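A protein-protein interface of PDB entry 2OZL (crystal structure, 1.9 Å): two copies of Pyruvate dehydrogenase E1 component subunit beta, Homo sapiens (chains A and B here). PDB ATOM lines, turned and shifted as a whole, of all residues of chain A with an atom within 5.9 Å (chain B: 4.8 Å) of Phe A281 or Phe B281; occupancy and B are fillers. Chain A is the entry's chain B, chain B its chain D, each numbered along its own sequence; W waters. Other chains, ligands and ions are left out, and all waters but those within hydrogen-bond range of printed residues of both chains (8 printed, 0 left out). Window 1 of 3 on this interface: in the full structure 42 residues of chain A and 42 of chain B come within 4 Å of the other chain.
Ala A145 touches none of the printed residues of chain B. Of the printed residues of chain B, Pro A279 touches Glu B286. Printed residues of chain A within 4 Å of Ala B146: Phe A281 (3.9 Å). Of the printed residues of chain A, Gln B280 touches His A150, Arg A254 and Glu A286. Printed residues of chain A within 4 Å of Phe B281: Ala A146, Gly A149, His A150, Ile A253, Met A256, Phe A281, Gly A282, Val A283 and Glu A286. The nearest printed residue of chain A that does not touch Phe B281 is Ala A145 (5.1 Å).
Hydrophobic or aromatic side chains of chain A within 4 Å of the printed part of chain B: Trp A147, His A150, Ile A253, Met A256, Trp A278, Phe A281 and Ala A285. Among the printed residues, 30 pairs touch across the chains.
The backbone carbonyl oxygen (O) of Gly A149 lies within hydrogen-bond range of the guanidinium group (NH1) of Arg A254 (2.8 Å). O of Pro A279 is in hydrogen-bond range of NH2 of Arg A306 (3.2 Å).
A ring nitrogen (ND1) of His A150 is in hydrogen-bond range of the backbone carbonyl oxygen of Gln B280, 2.6 Å away. The guanidinium group (NH1) of Arg A254 lies close to the side-chain amide nitrogen (NE2) of Gln B280, 3.3 Å away. A ring nitrogen (ND1) of His B150 is in hydrogen-bond range of the backbone carbonyl oxygen (O) of Gln A280. The backbone NH (N) of Phe A281 sits at hydrogen-bond distance from the side-chain carboxylate (OE1) of Glu B286 (2.8 Å). OE1 of Glu A286 is in hydrogen-bond range of N of Phe B281. OE1 of Glu B286 is in salt-bridge range of NH2 of Arg A306, at 3.0 Å. OE1 of Glu A286 lies close to O of Pro B279 (3.5 Å).
Phe B281 touches Ile A253. Pro A279 touches Glu B286 (O to OE1, 3.6 Å). CA of Gln A280 touches OE1 of Glu B286, 3.4 Å away. Phe A281 touches Ile B253. Met B256 touches Phe A281 (CE to CZ, 3.5 Å). Phe A281 touches Phe B281 (O to O, 3.99 Å). Phe A281 touches Val B283. CE1 of Phe B281 touches CA of Val A283 (3.6 Å). Ala B285 touches Ala A285 (O to O, 3.6 Å). Ala B285 touches Glu A286.
Water W8 lies within hydrogen-bond range of the side-chain amide oxygen (OE1) of Gln B280, the backbone NH (N) of Met A256 and the backbone carbonyl oxygen (O) of Ile A253. Water W1 bridges the backbone carbonyl oxygen of Phe A281 and the backbone carbonyl oxygen of Ala B146. Water W5 lies within hydrogen-bond range of NE2 of His B150 (2.9 Å) and N of Trp A278 (3.0 Å). Water W4 lies within hydrogen-bond range of the backbone carbonyl oxygen (O) of His A150, the backbone NH (N) of Gln B280 and the guanidinium group (NH1) of Arg A254. Water W6 bridges O of His B150 (2.9 Å) and N of Gln A280 (3.1 Å). Water W7 lies within hydrogen-bond range of N of Ala B146 (3.2 Å) and NE2 of His A150 (3.3 Å).
Gln A280 touches Glu B286, and with the chains exchanged Glu A286 touches Gln B280. Phe B281 touches its own counterpart, Phe A281. Ala B285 touches its own counterpart, Ala A285. Ala A285 touches Glu B286, and with the chains exchanged Glu A286 touches Ala B285. Of the 30 pairs that touch across the chains among the printed residues, 26 have their exchanged pair printed and touching as well.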
ATOM      1  N   ALA A 145     -18.055 -16.267  -5.330  1.00  0.00           N
ATOM      2  CA  ALA A 145     -19.493 -16.324  -5.079  1.00  0.00           C
ATOM      3  C   ALA A 145     -20.187 -15.010  -5.419  1.00  0.00           C
ATOM      4  O   ALA A 145     -21.220 -15.001  -6.095  1.00  0.00           O
ATOM      5  CB  ALA A 145     -19.756 -16.688  -3.618  1.00  0.00           C
ATOM      6  N   ALA A 146     -19.620 -13.904  -4.947  1.00  0.00           N
ATOM      7  CA  ALA A 146     -20.193 -12.581  -5.192  1.00  0.00           C
ATOM      8  C   ALA A 146     -20.164 -12.197  -6.666  1.00  0.00           C
ATOM      9  O   ALA A 146     -21.139 -11.668  -7.191  1.00  0.00           O
ATOM     10  CB  ALA A 146     -19.452 -11.531  -4.369  1.00  0.00           C
ATOM     11  N   TRP A 147     -19.039 -12.453  -7.325  1.00  0.00           N
ATOM     12  CA  TRP A 147     -18.893 -12.122  -8.740  1.00  0.00           C
ATOM     13  C   TRP A 147     -19.941 -12.795  -9.622  1.00  0.00           C
ATOM     14  O   TRP A 147     -20.627 -12.137 -10.409  1.00  0.00           O
ATOM     15  CB  TRP A 147     -17.499 -12.519  -9.232  1.00  0.00           C
ATOM     16  CG  TRP A 147     -16.456 -11.455  -9.084  1.00  0.00           C
ATOM     17  CD1 TRP A 147     -16.425 -10.444  -8.160  1.00  0.00           C
ATOM     18  CD2 TRP A 147     -15.263 -11.323  -9.861  1.00  0.00           C
ATOM     19  NE1 TRP A 147     -15.284  -9.694  -8.316  1.00  0.00           N
ATOM     20  CE2 TRP A 147     -14.553 -10.211  -9.354  1.00  0.00           C
ATOM     21  CE3 TRP A 147     -14.724 -12.037 -10.939  1.00  0.00           C
ATOM     22  CZ2 TRP A 147     -13.326  -9.796  -9.890  1.00  0.00           C
ATOM     23  CZ3 TRP A 147     -13.503 -11.627 -11.472  1.00  0.00           C
ATOM     24  CH2 TRP A 147     -12.818 -10.513 -10.944  1.00  0.00           C
ATOM     25  N   GLY A 149     -22.764 -14.507  -8.641  1.00  0.00           N
ATOM     26  CA  GLY A 149     -24.137 -14.296  -8.203  1.00  0.00           C
ATOM     27  C   GLY A 149     -24.698 -12.940  -8.605  1.00  0.00           C
ATOM     28  O   GLY A 149     -25.898 -12.682  -8.492  1.00  0.00           O
ATOM     29  N   HIS A 150     -23.813 -12.073  -9.082  1.00  0.00           N
ATOM     30  CA  HIS A 150     -24.147 -10.717  -9.512  1.00  0.00           C
ATOM     31  C   HIS A 150     -24.797 -10.698 -10.904  1.00  0.00           C
ATOM     32  O   HIS A 150     -25.544  -9.775 -11.231  1.00  0.00           O
ATOM     33  CB  HIS A 150     -22.837  -9.897  -9.518  1.00  0.00           C
ATOM     34  CG  HIS A 150     -22.975  -8.477  -9.982  1.00  0.00           C
ATOM     35  ND1 HIS A 150     -23.624  -7.506  -9.248  1.00  0.00           N
ATOM     36  CD2 HIS A 150     -22.486  -7.850 -11.079  1.00  0.00           C
ATOM     37  CE1 HIS A 150     -23.528  -6.345  -9.872  1.00  0.00           C
ATOM     38  NE2 HIS A 150     -22.842  -6.526 -10.986  1.00  0.00           N
ATOM     39  N   ILE A 253     -26.658 -19.312  -4.163  1.00  0.00           N
ATOM     40  CA  ILE A 253     -26.194 -17.926  -4.106  1.00  0.00           C
ATOM     41  C   ILE A 253     -27.091 -17.062  -4.994  1.00  0.00           C
ATOM     42  O   ILE A 253     -27.368 -15.909  -4.669  1.00  0.00           O
ATOM     43  CB  ILE A 253     -24.724 -17.797  -4.590  1.00  0.00           C
ATOM     44  CG1 ILE A 253     -23.801 -18.591  -3.664  1.00  0.00           C
ATOM     45  CG2 ILE A 253     -24.304 -16.325  -4.639  1.00  0.00           C
ATOM     46  CD1 ILE A 253     -23.865 -18.167  -2.211  1.00  0.00           C
ATOM     47  N   ARG A 254     -27.531 -17.630  -6.118  1.00  0.00           N
ATOM     48  CA  ARG A 254     -28.429 -16.939  -7.046  1.00  0.00           C
ATOM     49  C   ARG A 254     -29.314 -17.962  -7.764  1.00  0.00           C
ATOM     50  O   ARG A 254     -28.812 -18.847  -8.460  1.00  0.00           O
ATOM     51  CB  ARG A 254     -27.649 -16.140  -8.100  1.00  0.00           C
ATOM     52  CG  ARG A 254     -28.538 -15.152  -8.872  1.00  0.00           C
ATOM     53  CD  ARG A 254     -27.958 -14.733 -10.222  1.00  0.00           C
ATOM     54  NE  ARG A 254     -28.882 -13.857 -10.942  1.00  0.00           N
ATOM     55  CZ  ARG A 254     -28.943 -12.536 -10.793  1.00  0.00           C
ATOM     56  NH1 ARG A 254     -28.126 -11.913  -9.952  1.00  0.00           N
ATOM     57  NH2 ARG A 254     -29.837 -11.833 -11.475  1.00  0.00           N
ATOM     58  N   MET A 256     -30.959 -16.437  -4.420  1.00  0.00           N
ATOM     59  CA  MET A 256     -30.964 -16.797  -3.006  1.00  0.00           C
ATOM     60  C   MET A 256     -32.359 -16.845  -2.399  1.00  0.00           C
ATOM     61  O   MET A 256     -33.285 -16.173  -2.857  1.00  0.00           O
ATOM     62  CB  MET A 256     -30.082 -15.847  -2.192  1.00  0.00           C
ATOM     63  CG  MET A 256     -30.574 -14.416  -2.125  1.00  0.00           C
ATOM     64  SD  MET A 256     -29.587 -13.476  -0.946  1.00  0.00           S
ATOM     65  CE  MET A 256     -28.085 -13.200  -1.906  1.00  0.00           C
ATOM     66  N   TRP A 278     -13.882 -11.968   0.218  1.00  0.00           N
ATOM     67  CA  TRP A 278     -13.566 -10.595   0.596  1.00  0.00           C
ATOM     68  C   TRP A 278     -14.847  -9.864   0.989  1.00  0.00           C
ATOM     69  O   TRP A 278     -15.906 -10.074   0.397  1.00  0.00           O
ATOM     70  CB  TRP A 278     -12.849  -9.872  -0.548  1.00  0.00           C
ATOM     71  CG  TRP A 278     -11.494 -10.442  -0.852  1.00  0.00           C
ATOM     72  CD1 TRP A 278     -10.546 -10.831   0.056  1.00  0.00           C
ATOM     73  CD2 TRP A 278     -10.913 -10.642  -2.147  1.00  0.00           C
ATOM     74  NE1 TRP A 278      -9.415 -11.261  -0.593  1.00  0.00           N
ATOM     75  CE2 TRP A 278      -9.611 -11.155  -1.946  1.00  0.00           C
ATOM     76  CE3 TRP A 278     -11.362 -10.434  -3.457  1.00  0.00           C
ATOM     77  CZ2 TRP A 278      -8.754 -11.467  -3.008  1.00  0.00           C
ATOM     78  CZ3 TRP A 278     -10.509 -10.741  -4.516  1.00  0.00           C
ATOM     79  CH2 TRP A 278      -9.218 -11.253  -4.282  1.00  0.00           C
ATOM     80  N   PRO A 279     -14.753  -8.970   1.984  1.00  0.00           N
ATOM     81  CA  PRO A 279     -15.892  -8.205   2.491  1.00  0.00           C
ATOM     82  C   PRO A 279     -16.632  -7.213   1.601  1.00  0.00           C
ATOM     83  O   PRO A 279     -17.861  -7.262   1.516  1.00  0.00           O
ATOM     84  CB  PRO A 279     -15.322  -7.539   3.743  1.00  0.00           C
ATOM     85  CG  PRO A 279     -13.894  -7.288   3.367  1.00  0.00           C
ATOM     86  CD  PRO A 279     -13.502  -8.565   2.656  1.00  0.00           C
ATOM     87  N   GLN A 280     -15.910  -6.320   0.936  1.00  0.00           N
ATOM     88  CA  GLN A 280     -16.574  -5.304   0.127  1.00  0.00           C
ATOM     89  C   GLN A 280     -17.267  -5.822  -1.125  1.00  0.00           C
ATOM     90  O   GLN A 280     -16.642  -6.430  -1.993  1.00  0.00           O
ATOM     91  CB  GLN A 280     -15.584  -4.199  -0.226  1.00  0.00           C
ATOM     92  CG  GLN A 280     -14.876  -3.640   1.007  1.00  0.00           C
ATOM     93  CD  GLN A 280     -14.080  -2.397   0.707  1.00  0.00           C
ATOM     94  OE1 GLN A 280     -14.632  -1.392   0.261  1.00  0.00           O
ATOM     95  NE2 GLN A 280     -12.774  -2.453   0.950  1.00  0.00           N
ATOM     96  N   PHE A 281     -18.567  -5.562  -1.206  1.00  0.00           N
ATOM     97  CA  PHE A 281     -19.388  -5.996  -2.335  1.00  0.00           C
ATOM     98  C   PHE A 281     -19.497  -7.524  -2.325  1.00  0.00           C
ATOM     99  O   PHE A 281     -19.627  -8.157  -3.379  1.00  0.00           O
ATOM    100  CB  PHE A 281     -18.768  -5.521  -3.659  1.00  0.00           C
ATOM    101  CG  PHE A 281     -18.405  -4.058  -3.671  1.00  0.00           C
ATOM    102  CD1 PHE A 281     -19.387  -3.078  -3.812  1.00  0.00           C
ATOM    103  CD2 PHE A 281     -17.079  -3.660  -3.525  1.00  0.00           C
ATOM    104  CE1 PHE A 281     -19.051  -1.720  -3.805  1.00  0.00           C
ATOM    105  CE2 PHE A 281     -16.727  -2.303  -3.517  1.00  0.00           C
ATOM    106  CZ  PHE A 281     -17.714  -1.332  -3.657  1.00  0.00           C
ATOM    107  N   GLY A 282     -19.450  -8.106  -1.126  1.00  0.00           N
ATOM    108  CA  GLY A 282     -19.533  -9.554  -0.982  1.00  0.00           C
ATOM    109  C   GLY A 282     -20.937 -10.113  -0.813  1.00  0.00           C
ATOM    110  O   GLY A 282     -21.926  -9.397  -0.961  1.00  0.00           O
ATOM    111  N   VAL A 283     -21.027 -11.400  -0.494  1.00  0.00           N
ATOM    112  CA  VAL A 283     -22.317 -12.059  -0.308  1.00  0.00           C
ATOM    113  C   VAL A 283     -23.084 -11.443   0.863  1.00  0.00           C
ATOM    114  O   VAL A 283     -24.282 -11.148   0.753  1.00  0.00           O
ATOM    115  CB  VAL A 283     -22.126 -13.574  -0.063  1.00  0.00           C
ATOM    116  CG1 VAL A 283     -23.473 -14.251   0.144  1.00  0.00           C
ATOM    117  CG2 VAL A 283     -21.401 -14.195  -1.247  1.00  0.00           C
ATOM    118  N   GLY A 284     -22.386 -11.240   1.974  1.00  0.00           N
ATOM    119  CA  GLY A 284     -23.006 -10.650   3.148  1.00  0.00           C
ATOM    120  C   GLY A 284     -23.581  -9.263   2.906  1.00  0.00           C
ATOM    121  O   GLY A 284     -24.556  -8.873   3.550  1.00  0.00           O
ATOM    122  N   ALA A 285     -22.985  -8.510   1.985  1.00  0.00           N
ATOM    123  CA  ALA A 285     -23.470  -7.163   1.689  1.00  0.00           C
ATOM    124  C   ALA A 285     -24.876  -7.209   1.106  1.00  0.00           C
ATOM    125  O   ALA A 285     -25.742  -6.417   1.480  1.00  0.00           O
ATOM    126  CB  ALA A 285     -22.522  -6.462   0.718  1.00  0.00           C
ATOM    127  N   GLU A 286     -25.100  -8.141   0.186  1.00  0.00           N
ATOM    128  CA  GLU A 286     -26.401  -8.281  -0.447  1.00  0.00           C
ATOM    129  C   GLU A 286     -27.444  -8.738   0.560  1.00  0.00           C
ATOM    130  O   GLU A 286     -28.568  -8.249   0.552  1.00  0.00           O
ATOM    131  CB  GLU A 286     -26.317  -9.276  -1.605  1.00  0.00           C
ATOM    132  CG  GLU A 286     -27.618  -9.464  -2.372  1.00  0.00           C
ATOM    133  CD  GLU A 286     -28.185  -8.158  -2.900  1.00  0.00           C
ATOM    134  OE1 GLU A 286     -27.391  -7.237  -3.184  1.00  0.00           O
ATOM    135  OE2 GLU A 286     -29.426  -8.058  -3.045  1.00  0.00           O
ATOM    136  N   ILE A 287     -27.080  -9.680   1.424  1.00  0.00           N
ATOM    137  CA  ILE A 287     -28.023 -10.152   2.431  1.00  0.00           C
ATOM    138  C   ILE A 287     -28.404  -9.013   3.377  1.00  0.00           C
ATOM    139  O   ILE A 287     -29.575  -8.857   3.734  1.00  0.00           O
ATOM    140  CB  ILE A 287     -27.440 -11.311   3.266  1.00  0.00           C
ATOM    141  CG1 ILE A 287     -27.191 -12.527   2.372  1.00  0.00           C
ATOM    142  CG2 ILE A 287     -28.402 -11.674   4.391  1.00  0.00           C
ATOM    143  CD1 ILE A 287     -26.564 -13.701   3.097  1.00  0.00           C
ATOM    144  N   ARG A 306     -21.369  -8.476   9.597  1.00  0.00           N
ATOM    145  CA  ARG A 306     -20.759  -9.427   8.673  1.00  0.00           C
ATOM    146  C   ARG A 306     -19.418  -9.999   9.123  1.00  0.00           C
ATOM    147  O   ARG A 306     -18.553  -9.267   9.609  1.00  0.00           O
ATOM    148  CB  ARG A 306     -20.553  -8.758   7.307  1.00  0.00           C
ATOM    149  CG  ARG A 306     -21.822  -8.254   6.638  1.00  0.00           C
ATOM    150  CD  ARG A 306     -21.505  -7.568   5.315  1.00  0.00           C
ATOM    151  NE  ARG A 306     -20.781  -6.320   5.525  1.00  0.00           N
ATOM    152  CZ  ARG A 306     -20.176  -5.626   4.567  1.00  0.00           C
ATOM    153  NH1 ARG A 306     -19.549  -4.495   4.870  1.00  0.00           N
ATOM    154  NH2 ARG A 306     -20.182  -6.062   3.314  1.00  0.00           N
ATOM    155  N   ALA B 146     -18.688  -2.899  -9.039  1.00  0.00           N
ATOM    156  CA  ALA B 146     -18.682  -3.828  -7.905  1.00  0.00           C
ATOM    157  C   ALA B 146     -17.633  -4.922  -8.043  1.00  0.00           C
ATOM    158  O   ALA B 146     -16.960  -5.272  -7.070  1.00  0.00           O
ATOM    159  CB  ALA B 146     -20.064  -4.456  -7.732  1.00  0.00           C
ATOM    160  N   GLY B 149     -14.171  -3.216  -7.491  1.00  0.00           N
ATOM    161  CA  GLY B 149     -14.099  -2.630  -6.160  1.00  0.00           C
ATOM    162  C   GLY B 149     -13.964  -3.677  -5.072  1.00  0.00           C
ATOM    163  O   GLY B 149     -13.576  -3.377  -3.944  1.00  0.00           O
ATOM    164  N   HIS B 150     -14.283  -4.912  -5.434  1.00  0.00           N
ATOM    165  CA  HIS B 150     -14.245  -6.073  -4.547  1.00  0.00           C
ATOM    166  C   HIS B 150     -12.825  -6.569  -4.248  1.00  0.00           C
ATOM    167  O   HIS B 150     -12.603  -7.233  -3.239  1.00  0.00           O
ATOM    168  CB  HIS B 150     -15.056  -7.197  -5.226  1.00  0.00           C
ATOM    169  CG  HIS B 150     -15.134  -8.482  -4.454  1.00  0.00           C
ATOM    170  ND1 HIS B 150     -15.875  -8.620  -3.299  1.00  0.00           N
ATOM    171  CD2 HIS B 150     -14.632  -9.711  -4.725  1.00  0.00           C
ATOM    172  CE1 HIS B 150     -15.831  -9.877  -2.895  1.00  0.00           C
ATOM    173  NE2 HIS B 150     -15.082 -10.560  -3.743  1.00  0.00           N
ATOM    174  N   ILE B 253     -14.545   4.172  -5.882  1.00  0.00           N
ATOM    175  CA  ILE B 253     -15.314   2.971  -5.556  1.00  0.00           C
ATOM    176  C   ILE B 253     -14.536   2.201  -4.493  1.00  0.00           C
ATOM    177  O   ILE B 253     -15.121   1.657  -3.549  1.00  0.00           O
ATOM    178  CB  ILE B 253     -15.510   2.085  -6.809  1.00  0.00           C
ATOM    179  CG1 ILE B 253     -16.228   2.884  -7.905  1.00  0.00           C
ATOM    180  CG2 ILE B 253     -16.306   0.840  -6.455  1.00  0.00           C
ATOM    181  CD1 ILE B 253     -17.606   3.387  -7.515  1.00  0.00           C
ATOM    182  N   MET B 256     -13.766   3.465  -0.967  1.00  0.00           N
ATOM    183  CA  MET B 256     -14.833   4.454  -0.909  1.00  0.00           C
ATOM    184  C   MET B 256     -14.757   5.312   0.354  1.00  0.00           C
ATOM    185  O   MET B 256     -14.266   4.873   1.397  1.00  0.00           O
ATOM    186  CB  MET B 256     -16.211   3.782  -1.005  1.00  0.00           C
ATOM    187  CG  MET B 256     -16.571   2.859   0.146  1.00  0.00           C
ATOM    188  SD  MET B 256     -18.323   2.385   0.073  1.00  0.00           S
ATOM    189  CE  MET B 256     -18.299   1.266  -1.339  1.00  0.00           C
ATOM    190  N   PRO B 279     -28.351  -4.880  -9.436  1.00  0.00           N
ATOM    191  CA  PRO B 279     -28.602  -4.793  -7.992  1.00  0.00           C
ATOM    192  C   PRO B 279     -27.894  -5.746  -7.031  1.00  0.00           C
ATOM    193  O   PRO B 279     -27.255  -5.302  -6.077  1.00  0.00           O
ATOM    194  CB  PRO B 279     -30.123  -4.914  -7.907  1.00  0.00           C
ATOM    195  CG  PRO B 279     -30.437  -5.848  -9.030  1.00  0.00           C
ATOM    196  CD  PRO B 279     -29.557  -5.338 -10.155  1.00  0.00           C
ATOM    197  N   GLN B 280     -27.996  -7.047  -7.276  1.00  0.00           N
ATOM    198  CA  GLN B 280     -27.404  -8.017  -6.368  1.00  0.00           C
ATOM    199  C   GLN B 280     -25.881  -7.987  -6.284  1.00  0.00           C
ATOM    200  O   GLN B 280     -25.182  -8.158  -7.280  1.00  0.00           O
ATOM    201  CB  GLN B 280     -27.906  -9.416  -6.727  1.00  0.00           C
ATOM    202  CG  GLN B 280     -29.432  -9.474  -6.820  1.00  0.00           C
ATOM    203  CD  GLN B 280     -29.973 -10.889  -6.875  1.00  0.00           C
ATOM    204  OE1 GLN B 280     -29.750 -11.682  -5.963  1.00  0.00           O
ATOM    205  NE2 GLN B 280     -30.690 -11.209  -7.944  1.00  0.00           N
ATOM    206  N   PHE B 281     -25.381  -7.761  -5.073  1.00  0.00           N
ATOM    207  CA  PHE B 281     -23.944  -7.696  -4.817  1.00  0.00           C
ATOM    208  C   PHE B 281     -23.355  -6.476  -5.519  1.00  0.00           C
ATOM    209  O   PHE B 281     -22.197  -6.485  -5.934  1.00  0.00           O
ATOM    210  CB  PHE B 281     -23.258  -8.981  -5.313  1.00  0.00           C
ATOM    211  CG  PHE B 281     -23.943 -10.240  -4.863  1.00  0.00           C
ATOM    212  CD1 PHE B 281     -23.876 -10.651  -3.537  1.00  0.00           C
ATOM    213  CD2 PHE B 281     -24.704 -10.990  -5.758  1.00  0.00           C
ATOM    214  CE1 PHE B 281     -24.561 -11.794  -3.108  1.00  0.00           C
ATOM    215  CE2 PHE B 281     -25.391 -12.130  -5.342  1.00  0.00           C
ATOM    216  CZ  PHE B 281     -25.323 -12.534  -4.018  1.00  0.00           C
ATOM    217  N   GLY B 282     -24.162  -5.426  -5.642  1.00  0.00           N
ATOM    218  CA  GLY B 282     -23.711  -4.213  -6.298  1.00  0.00           C
ATOM    219  C   GLY B 282     -23.115  -3.178  -5.363  1.00  0.00           C
ATOM    220  O   GLY B 282     -22.885  -3.445  -4.182  1.00  0.00           O
ATOM    221  N   VAL B 283     -22.871  -1.986  -5.898  1.00  0.00           N
ATOM    222  CA  VAL B 283     -22.286  -0.899  -5.125  1.00  0.00           C
ATOM    223  C   VAL B 283     -23.213  -0.461  -3.993  1.00  0.00           C
ATOM    224  O   VAL B 283     -22.762  -0.188  -2.881  1.00  0.00           O
ATOM    225  CB  VAL B 283     -21.975   0.319  -6.029  1.00  0.00           C
ATOM    226  CG1 VAL B 283     -21.434   1.472  -5.188  1.00  0.00           C
ATOM    227  CG2 VAL B 283     -20.958  -0.071  -7.095  1.00  0.00           C
ATOM    228  N   ALA B 285     -25.330  -2.245  -2.391  1.00  0.00           N
ATOM    229  CA  ALA B 285     -25.359  -3.257  -1.341  1.00  0.00           C
ATOM    230  C   ALA B 285     -24.273  -2.990  -0.306  1.00  0.00           C
ATOM    231  O   ALA B 285     -24.518  -3.058   0.904  1.00  0.00           O
ATOM    232  CB  ALA B 285     -25.185  -4.648  -1.947  1.00  0.00           C
ATOM    233  N   GLU B 286     -23.070  -2.677  -0.779  1.00  0.00           N
ATOM    234  CA  GLU B 286     -21.952  -2.402   0.117  1.00  0.00           C
ATOM    235  C   GLU B 286     -22.201  -1.150   0.960  1.00  0.00           C
ATOM    236  O   GLU B 286     -21.977  -1.154   2.171  1.00  0.00           O
ATOM    237  CB  GLU B 286     -20.660  -2.239  -0.691  1.00  0.00           C
ATOM    238  CG  GLU B 286     -19.418  -1.981   0.148  1.00  0.00           C
ATOM    239  CD  GLU B 286     -19.144  -3.077   1.159  1.00  0.00           C
ATOM    240  OE1 GLU B 286     -19.631  -4.215   0.965  1.00  0.00           O
ATOM    241  OE2 GLU B 286     -18.427  -2.806   2.147  1.00  0.00           O
HETATM  242  O   HOH W   1     -18.352  -8.232  -5.890  1.00  0.00           O
HETATM  243  O   HOH W   2     -16.693 -12.845  -5.420  1.00  0.00           O
HETATM  244  O   HOH W   3     -14.134   0.687  -1.090  1.00  0.00           O
HETATM  245  O   HOH W   4     -27.858  -8.693  -9.889  1.00  0.00           O
HETATM  246  O   HOH W   5     -13.789 -12.882  -2.644  1.00  0.00           O
HETATM  247  O   HOH W   6     -13.194  -6.423  -0.478  1.00  0.00           O
HETATM  248  O   HOH W   7     -19.869  -5.064 -11.022  1.00  0.00           O
HETATM  249  O   HOH W   8     -29.655 -14.083  -5.566  1.00  0.00           O
